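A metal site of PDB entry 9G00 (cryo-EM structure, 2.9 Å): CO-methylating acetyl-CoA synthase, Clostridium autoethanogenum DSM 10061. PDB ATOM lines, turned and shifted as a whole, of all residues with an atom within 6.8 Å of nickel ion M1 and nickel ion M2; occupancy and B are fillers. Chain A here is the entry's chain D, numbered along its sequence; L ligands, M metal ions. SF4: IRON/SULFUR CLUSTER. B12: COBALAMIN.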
ATOM      1  N   LEU A 487      -0.309  -4.559 -21.386  1.00  0.00           N
ATOM      2  CA  LEU A 487      -1.583  -4.885 -20.774  1.00  0.00           C
ATOM      3  C   LEU A 487      -2.733  -4.009 -21.267  1.00  0.00           C
ATOM      4  O   LEU A 487      -3.893  -4.311 -20.959  1.00  0.00           O
ATOM      5  CB  LEU A 487      -1.493  -4.778 -19.254  1.00  0.00           C
ATOM      6  CG  LEU A 487      -1.724  -6.062 -18.464  1.00  0.00           C
ATOM      7  CD1 LEU A 487      -1.653  -5.799 -16.980  1.00  0.00           C
ATOM      8  CD2 LEU A 487      -3.059  -6.690 -18.810  1.00  0.00           C
ATOM      9  N   CYS A 488      -2.444  -2.935 -21.986  1.00  0.00           N
ATOM     10  CA  CYS A 488      -3.478  -2.085 -22.561  1.00  0.00           C
ATOM     11  C   CYS A 488      -3.771  -2.416 -24.009  1.00  0.00           C
ATOM     12  O   CYS A 488      -4.529  -1.685 -24.662  1.00  0.00           O
ATOM     13  CB  CYS A 488      -3.090  -0.605 -22.443  1.00  0.00           C
ATOM     14  SG  CYS A 488      -3.213   0.074 -20.769  1.00  0.00           S
ATOM     15  N   GLN A 489      -3.176  -3.487 -24.545  1.00  0.00           N
ATOM     16  CA  GLN A 489      -3.465  -3.896 -25.913  1.00  0.00           C
ATOM     17  C   GLN A 489      -4.843  -4.518 -26.063  1.00  0.00           C
ATOM     18  O   GLN A 489      -5.245  -4.813 -27.195  1.00  0.00           O
ATOM     19  CB  GLN A 489      -2.403  -4.873 -26.406  1.00  0.00           C
ATOM     20  CG  GLN A 489      -1.050  -4.239 -26.598  1.00  0.00           C
ATOM     21  CD  GLN A 489      -0.116  -5.100 -27.420  1.00  0.00           C
ATOM     22  OE1 GLN A 489      -0.509  -6.152 -27.912  1.00  0.00           O
ATOM     23  NE2 GLN A 489       1.124  -4.665 -27.554  1.00  0.00           N
ATOM     24  N   PHE A 491      -7.518  -2.997 -25.837  1.00  0.00           N
ATOM     25  CA  PHE A 491      -8.271  -2.015 -26.607  1.00  0.00           C
ATOM     26  C   PHE A 491      -7.416  -1.131 -27.498  1.00  0.00           C
ATOM     27  O   PHE A 491      -7.965  -0.407 -28.328  1.00  0.00           O
ATOM     28  CB  PHE A 491      -9.086  -1.109 -25.674  1.00  0.00           C
ATOM     29  CG  PHE A 491      -8.246  -0.226 -24.797  1.00  0.00           C
ATOM     30  CD1 PHE A 491      -7.687  -0.729 -23.632  1.00  0.00           C
ATOM     31  CD2 PHE A 491      -8.031   1.094 -25.116  1.00  0.00           C
ATOM     32  CE1 PHE A 491      -6.927   0.080 -22.826  1.00  0.00           C
ATOM     33  CE2 PHE A 491      -7.273   1.895 -24.298  1.00  0.00           C
ATOM     34  CZ  PHE A 491      -6.722   1.381 -23.158  1.00  0.00           C
ATOM     35  N   ALA A 492      -6.087  -1.172 -27.354  1.00  0.00           N
ATOM     36  CA  ALA A 492      -5.165  -0.438 -28.219  1.00  0.00           C
ATOM     37  C   ALA A 492      -4.143  -1.449 -28.725  1.00  0.00           C
ATOM     38  O   ALA A 492      -3.020  -1.526 -28.220  1.00  0.00           O
ATOM     39  CB  ALA A 492      -4.483   0.704 -27.466  1.00  0.00           C
ATOM     40  N   HIS A 495      -0.295  -0.674 -29.176  1.00  0.00           N
ATOM     41  CA  HIS A 495       0.350   0.081 -28.118  1.00  0.00           C
ATOM     42  C   HIS A 495       1.315  -0.791 -27.319  1.00  0.00           C
ATOM     43  O   HIS A 495       0.928  -1.851 -26.807  1.00  0.00           O
ATOM     44  CB  HIS A 495      -0.696   0.660 -27.172  1.00  0.00           C
ATOM     45  CG  HIS A 495      -0.100   1.362 -25.987  1.00  0.00           C
ATOM     46  ND1 HIS A 495       0.764   2.423 -26.116  1.00  0.00           N
ATOM     47  CD2 HIS A 495      -0.238   1.135 -24.660  1.00  0.00           C
ATOM     48  CE1 HIS A 495       1.128   2.833 -24.916  1.00  0.00           C
ATOM     49  NE2 HIS A 495       0.536   2.073 -24.018  1.00  0.00           N
ATOM     50  N   CYS A 497       4.170  -0.034 -24.190  1.00  0.00           N
ATOM     51  CA  CYS A 497       4.746   0.906 -23.236  1.00  0.00           C
ATOM     52  C   CYS A 497       6.181   0.480 -22.930  1.00  0.00           C
ATOM     53  O   CYS A 497       6.402  -0.638 -22.461  1.00  0.00           O
ATOM     54  CB  CYS A 497       3.939   0.957 -21.941  1.00  0.00           C
ATOM     55  SG  CYS A 497       2.531   2.078 -21.959  1.00  0.00           S
ATOM     56  N   LEU A 506       2.295   5.014 -18.871  1.00  0.00           N
ATOM     57  CA  LEU A 506       1.343   6.094 -19.098  1.00  0.00           C
ATOM     58  C   LEU A 506       0.288   6.134 -18.015  1.00  0.00           C
ATOM     59  O   LEU A 506      -0.103   7.220 -17.559  1.00  0.00           O
ATOM     60  CB  LEU A 506       0.691   5.951 -20.471  1.00  0.00           C
ATOM     61  CG  LEU A 506       1.623   5.708 -21.652  1.00  0.00           C
ATOM     62  CD1 LEU A 506       0.837   5.817 -22.937  1.00  0.00           C
ATOM     63  CD2 LEU A 506       2.787   6.683 -21.656  1.00  0.00           C
ATOM     64  N   CYS A 507      -0.192   4.974 -17.576  1.00  0.00           N
ATOM     65  CA  CYS A 507      -1.188   4.944 -16.514  1.00  0.00           C
ATOM     66  C   CYS A 507      -0.610   5.401 -15.187  1.00  0.00           C
ATOM     67  O   CYS A 507      -1.382   5.789 -14.303  1.00  0.00           O
ATOM     68  CB  CYS A 507      -1.739   3.531 -16.376  1.00  0.00           C
ATOM     69  SG  CYS A 507      -0.473   2.263 -16.202  1.00  0.00           S
ATOM     70  N   SER A 573       0.079   5.913 -27.430  1.00  0.00           N
ATOM     71  CA  SER A 573      -0.704   6.099 -26.225  1.00  0.00           C
ATOM     72  C   SER A 573      -1.957   5.230 -26.294  1.00  0.00           C
ATOM     73  O   SER A 573      -2.536   5.059 -27.366  1.00  0.00           O
ATOM     74  CB  SER A 573      -1.117   7.555 -26.055  1.00  0.00           C
ATOM     75  OG  SER A 573       0.010   8.415 -26.086  1.00  0.00           O
ATOM     76  N   CYS A 574      -2.349   4.690 -25.145  1.00  0.00           N
ATOM     77  CA  CYS A 574      -3.530   3.825 -25.095  1.00  0.00           C
ATOM     78  C   CYS A 574      -4.784   4.615 -24.765  1.00  0.00           C
ATOM     79  O   CYS A 574      -5.674   4.760 -25.615  1.00  0.00           O
ATOM     80  CB  CYS A 574      -3.319   2.711 -24.063  1.00  0.00           C
ATOM     81  SG  CYS A 574      -2.331   3.194 -22.638  1.00  0.00           S
ATOM     82  N   GLY A 575      -4.835   5.239 -23.596  1.00  0.00           N
ATOM     83  CA  GLY A 575      -6.059   5.896 -23.171  1.00  0.00           C
ATOM     84  C   GLY A 575      -6.217   5.985 -21.675  1.00  0.00           C
ATOM     85  O   GLY A 575      -7.160   6.601 -21.170  1.00  0.00           O
ATOM     86  N   CYS A 576      -5.294   5.356 -20.958  1.00  0.00           N
ATOM     87  CA  CYS A 576      -5.235   5.442 -19.507  1.00  0.00           C
ATOM     88  C   CYS A 576      -4.491   6.659 -19.006  1.00  0.00           C
ATOM     89  O   CYS A 576      -4.535   6.940 -17.797  1.00  0.00           O
ATOM     90  CB  CYS A 576      -4.559   4.184 -18.979  1.00  0.00           C
ATOM     91  SG  CYS A 576      -3.194   3.631 -20.015  1.00  0.00           S
ATOM     92  N   PHE A 577      -3.841   7.403 -19.892  1.00  0.00           N
ATOM     93  CA  PHE A 577      -3.062   8.565 -19.475  1.00  0.00           C
ATOM     94  C   PHE A 577      -3.939   9.612 -18.806  1.00  0.00           C
ATOM     95  O   PHE A 577      -5.069   9.857 -19.229  1.00  0.00           O
ATOM     96  CB  PHE A 577      -2.342   9.166 -20.683  1.00  0.00           C
ATOM     97  CG  PHE A 577      -3.204   9.281 -21.906  1.00  0.00           C
ATOM     98  CD1 PHE A 577      -4.095  10.324 -22.057  1.00  0.00           C
ATOM     99  CD2 PHE A 577      -3.132   8.333 -22.904  1.00  0.00           C
ATOM    100  CE1 PHE A 577      -4.889  10.414 -23.179  1.00  0.00           C
ATOM    101  CE2 PHE A 577      -3.917   8.426 -24.022  1.00  0.00           C
ATOM    102  CZ  PHE A 577      -4.797   9.464 -24.166  1.00  0.00           C
ATOM    103  N   ARG A 595      -6.686  14.998 -17.207  1.00  0.00           N
ATOM    104  CA  ARG A 595      -7.981  14.405 -17.540  1.00  0.00           C
ATOM    105  C   ARG A 595      -9.125  15.127 -16.832  1.00  0.00           C
ATOM    106  O   ARG A 595     -10.172  15.376 -17.444  1.00  0.00           O
ATOM    107  CB  ARG A 595      -7.976  12.927 -17.192  1.00  0.00           C
ATOM    108  CG  ARG A 595      -9.293  12.222 -17.463  1.00  0.00           C
ATOM    109  CD  ARG A 595      -9.174  10.714 -17.268  1.00  0.00           C
ATOM    110  NE  ARG A 595      -8.338  10.098 -18.283  1.00  0.00           N
ATOM    111  CZ  ARG A 595      -8.777   9.679 -19.463  1.00  0.00           C
ATOM    112  NH1 ARG A 595     -10.046   9.811 -19.817  1.00  0.00           N
ATOM    113  NH2 ARG A 595      -7.918   9.116 -20.316  1.00  0.00           N
ATOM    114  N   GLY A 615      -4.817   8.820 -28.293  1.00  0.00           N
ATOM    115  CA  GLY A 615      -4.987   7.462 -27.836  1.00  0.00           C
ATOM    116  C   GLY A 615      -5.214   6.480 -28.963  1.00  0.00           C
ATOM    117  O   GLY A 615      -5.268   6.827 -30.144  1.00  0.00           O
HETATM  118 FE1  SF4 L   1       0.785  -1.576 -19.033  1.00  0.00          FE
HETATM  119 FE2  SF4 L   1       1.439   0.719 -20.373  1.00  0.00          FE
HETATM  120 FE3  SF4 L   1       0.357   0.861 -17.866  1.00  0.00          FE
HETATM  121 FE4  SF4 L   1      -1.183   0.054 -19.986  1.00  0.00          FE
HETATM  122  S1  SF4 L   1      -0.232   2.108 -19.691  1.00  0.00           S
HETATM  123  S2  SF4 L   1      -1.084  -0.911 -17.924  1.00  0.00           S
HETATM  124  S3  SF4 L   1       0.345  -1.097 -21.219  1.00  0.00           S
HETATM  125  S4  SF4 L   1       2.365  -0.048 -18.436  1.00  0.00           S
HETATM  126 CO   B12 L   2      -7.358   0.992 -16.673  1.00  0.00          CO
HETATM  127  N21 B12 L   2      -6.437   0.219 -15.237  1.00  0.00           N
HETATM  128  N22 B12 L   2      -7.118   2.746 -15.911  1.00  0.00           N
HETATM  129  N23 B12 L   2      -8.281   1.481 -18.205  1.00  0.00           N
HETATM  130  N24 B12 L   2      -7.447  -0.837 -17.220  1.00  0.00           N
HETATM  131  C1  B12 L   2      -6.355  -1.259 -15.114  1.00  0.00           C
HETATM  132  C20 B12 L   2      -7.615  -1.785 -14.342  1.00  0.00           C
HETATM  133  C2  B12 L   2      -5.042  -1.468 -14.277  1.00  0.00           C
HETATM  134  C25 B12 L   2      -4.918  -2.887 -13.623  1.00  0.00           C
HETATM  135  C26 B12 L   2      -3.818  -1.150 -15.157  1.00  0.00           C
HETATM  136  C27 B12 L   2      -2.506  -1.252 -14.381  1.00  0.00           C
HETATM  137  O28 B12 L   2      -2.165  -2.188 -13.658  1.00  0.00           O
HETATM  138  N29 B12 L   2      -1.702  -0.197 -14.551  1.00  0.00           N
HETATM  139  C3  B12 L   2      -5.215  -0.307 -13.257  1.00  0.00           C
HETATM  140  C30 B12 L   2      -5.965  -0.482 -11.900  1.00  0.00           C
HETATM  141  C31 B12 L   2      -5.108  -0.090 -10.651  1.00  0.00           C
HETATM  142  C32 B12 L   2      -5.908   0.240  -9.397  1.00  0.00           C
HETATM  143  O34 B12 L   2      -6.976   0.861  -9.471  1.00  0.00           O
HETATM  144  N33 B12 L   2      -5.427  -0.167  -8.216  1.00  0.00           N
HETATM  145  C4  B12 L   2      -5.923   0.744 -14.135  1.00  0.00           C
HETATM  146  C5  B12 L   2      -5.897   2.169 -13.861  1.00  0.00           C
HETATM  147  C35 B12 L   2      -5.205   2.528 -12.577  1.00  0.00           C
HETATM  148  C6  B12 L   2      -6.476   3.110 -14.701  1.00  0.00           C
HETATM  149  C7  B12 L   2      -6.522   4.626 -14.523  1.00  0.00           C
HETATM  150  C36 B12 L   2      -7.158   5.065 -13.184  1.00  0.00           C
HETATM  151  C37 B12 L   2      -5.055   5.206 -14.664  1.00  0.00           C
HETATM  152  C38 B12 L   2      -5.012   6.751 -14.398  1.00  0.00           C
HETATM  153  O39 B12 L   2      -4.592   7.128 -13.323  1.00  0.00           O
HETATM  154  N40 B12 L   2      -5.403   7.627 -15.319  1.00  0.00           N
HETATM  155  C8  B12 L   2      -7.317   5.114 -15.742  1.00  0.00           C
HETATM  156  C41 B12 L   2      -8.689   5.830 -15.399  1.00  0.00           C
HETATM  157  C42 B12 L   2      -9.304   6.612 -16.568  1.00  0.00           C
HETATM  158  C43 B12 L   2     -10.327   7.595 -16.114  1.00  0.00           C
HETATM  159  O44 B12 L   2     -10.249   8.095 -14.973  1.00  0.00           O
HETATM  160  N45 B12 L   2     -11.357   7.947 -16.903  1.00  0.00           N
HETATM  161  C9  B12 L   2      -7.568   3.823 -16.506  1.00  0.00           C
HETATM  162  C10 B12 L   2      -8.252   3.808 -17.683  1.00  0.00           C
HETATM  163  C11 B12 L   2      -8.587   2.772 -18.472  1.00  0.00           C
HETATM  164  C12 B12 L   2      -9.286   2.957 -19.809  1.00  0.00           C
HETATM  165  C46 B12 L   2      -8.263   3.704 -20.728  1.00  0.00           C
HETATM  166  C47 B12 L   2     -10.580   3.800 -19.641  1.00  0.00           C
HETATM  167  C13 B12 L   2      -9.519   1.529 -20.240  1.00  0.00           C
HETATM  168  C48 B12 L   2     -11.024   1.047 -20.225  1.00  0.00           C
HETATM  169  C49 B12 L   2     -11.616   1.075 -21.642  1.00  0.00           C
HETATM  170  C50 B12 L   2     -12.719   0.013 -21.677  1.00  0.00           C
HETATM  171  O51 B12 L   2     -13.575  -0.080 -20.722  1.00  0.00           O
HETATM  172  N52 B12 L   2     -12.691  -0.766 -22.692  1.00  0.00           N
HETATM  173  C14 B12 L   2      -8.764   0.702 -19.216  1.00  0.00           C
HETATM  174  C15 B12 L   2      -8.645  -0.673 -19.285  1.00  0.00           C
HETATM  175  C53 B12 L   2      -9.232  -1.446 -20.459  1.00  0.00           C
HETATM  176  C16 B12 L   2      -8.030  -1.410 -18.231  1.00  0.00           C
HETATM  177  C17 B12 L   2      -7.691  -2.922 -18.241  1.00  0.00           C
HETATM  178  C54 B12 L   2      -6.649  -3.000 -19.391  1.00  0.00           C
HETATM  179  C55 B12 L   2      -8.789  -3.920 -18.521  1.00  0.00           C
HETATM  180  C56 B12 L   2     -10.104  -3.783 -17.741  1.00  0.00           C
HETATM  181  C57 B12 L   2     -10.993  -5.005 -18.017  1.00  0.00           C
HETATM  182  O58 B12 L   2     -11.756  -5.011 -18.971  1.00  0.00           O
HETATM  183  N59 B12 L   2     -10.835  -6.040 -17.218  1.00  0.00           N
HETATM  184  C18 B12 L   2      -7.041  -3.130 -16.878  1.00  0.00           C
HETATM  185  C60 B12 L   2      -5.989  -4.275 -16.744  1.00  0.00           C
HETATM  186  C61 B12 L   2      -6.312  -5.284 -15.641  1.00  0.00           C
HETATM  187  O63 B12 L   2      -7.458  -5.423 -15.190  1.00  0.00           O
HETATM  188  N62 B12 L   2      -5.261  -5.984 -15.231  1.00  0.00           N
HETATM  189  C19 B12 L   2      -6.464  -1.760 -16.573  1.00  0.00           C
HETATM  190  C1P B12 L   2     -11.579  -7.303 -17.394  1.00  0.00           C
HETATM  191  C2P B12 L   2     -13.056  -7.191 -17.009  1.00  0.00           C
HETATM  192  C3P B12 L   2     -13.886  -8.306 -17.662  1.00  0.00           C
HETATM  193  O3  B12 L   2     -13.110  -7.427 -15.576  1.00  0.00           O
HETATM  194  O4  B12 L   2     -14.819  -5.575 -15.456  1.00  0.00           O
HETATM  195  O5  B12 L   2     -13.697  -6.528 -13.311  1.00  0.00           O
HETATM  196  P   B12 L   2     -14.277  -6.717 -14.703  1.00  0.00           P
HETATM  197  O2  B12 L   2     -15.436  -7.869 -14.561  1.00  0.00           O
HETATM  198  C3R B12 L   2     -15.199  -9.113 -13.971  1.00  0.00           C
HETATM  199  C2R B12 L   2     -15.440  -9.158 -12.465  1.00  0.00           C
HETATM  200  O7R B12 L   2     -15.739  -7.935 -11.864  1.00  0.00           O
HETATM  201  C1R B12 L   2     -16.587 -10.199 -12.262  1.00  0.00           C
HETATM  202  O6R B12 L   2     -16.689 -10.892 -13.473  1.00  0.00           O
HETATM  203  C4R B12 L   2     -16.317 -10.030 -14.560  1.00  0.00           C
HETATM  204  C5R B12 L   2     -15.884 -10.864 -15.762  1.00  0.00           C
HETATM  205  O8R B12 L   2     -14.897 -11.844 -15.309  1.00  0.00           O
HETATM  206  N1B B12 L   2     -17.913  -9.669 -11.919  1.00  0.00           N
HETATM  207  C8B B12 L   2     -18.789 -10.345 -11.101  1.00  0.00           C
HETATM  208  C2B B12 L   2     -18.539  -8.556 -12.280  1.00  0.00           C
HETATM  209  N3B B12 L   2     -19.743  -8.451 -11.746  1.00  0.00           N
HETATM  210  C9B B12 L   2     -19.946  -9.606 -10.973  1.00  0.00           C
HETATM  211  C4B B12 L   2     -20.988 -10.097 -10.173  1.00  0.00           C
HETATM  212  C5B B12 L   2     -20.858 -11.319  -9.517  1.00  0.00           C
HETATM  213  C5M B12 L   2     -21.972 -11.871  -8.660  1.00  0.00           C
HETATM  214  C6B B12 L   2     -19.682 -12.085  -9.640  1.00  0.00           C
HETATM  215  C6M B12 L   2     -19.447 -13.395  -8.989  1.00  0.00           C
HETATM  216  C7B B12 L   2     -18.643 -11.576 -10.447  1.00  0.00           C
HETATM  217 NI    NI M   1      -3.998   4.428 -21.940  1.00  0.00          NI
HETATM  218 NI    NI M   2      -2.286   2.006 -20.864  1.00  0.00          NI
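Nickel ion M2 is bound by SG of Cys 576, 2.0 Å away.
Nickel ion M2 is bound by SG of Cys 574, at 2.1 Å.
Nickel ion M2 is bound by SG of Cys 488 (2.1 Å).
S1 of SF4 L1 binds nickel ion M2, 2.4 Å away.
The guanidinium group (NH2) of Arg 595 is in hydrogen-bond range of the backbone carbonyl oxygen (O) of Phe 577 (3.1 Å).
O of Gly 575 is in hydrogen-bond range of NH2 of Arg 595, at 2.8 Å.
NE2 of His 495 lies close to SG of Cys 574, at 3.4 Å.
Residues that only touch nickel ion M1: Phe 577 (3.6 Å).
SG of Cys 488 binds FE4 of SF4 L1.
S3 of SF4 L1 lies close to N of Leu 487 (3.5 Å).
The side-chain sulfur of Cys 507 lies close to a nitrogen (N29) of B12 L2 (3.2 Å).
The side-chain sulfur (SG) of Cys 507 is bound to an iron atom (FE3) of SF4 L1 (2.3 Å).
The backbone NH (N) of Cys 507 lies close to a sulfur (S1) of SF4 L1 (3.6 Å).
N of Cys 488 sits close to S3 of SF4 L1 (3.4 Å).
The backbone carbonyl oxygen of Cys 576 is in hydrogen-bond range of a nitrogen (N40) of B12 L2, 2.7 Å away.
The side-chain sulfur (SG) of Cys 497 binds an iron atom (FE2) of SF4 L1 (2.4 Å).
Within 4 Å of nickel ion M2: Cys 488, Cys 574 and Cys 576.
S2 of SF4 L1 sits close to N29 of B12 L2 (3.5 Å).
Nickel ion M1 is bound by the backbone nitrogen of Cys 576 (1.9 Å), the backbone nitrogen of Gly 575 (2.0 Å), the side-chain sulfur of Cys 574 (2.2 Å) and the side-chain sulfur of Cys 576 (2.2 Å).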
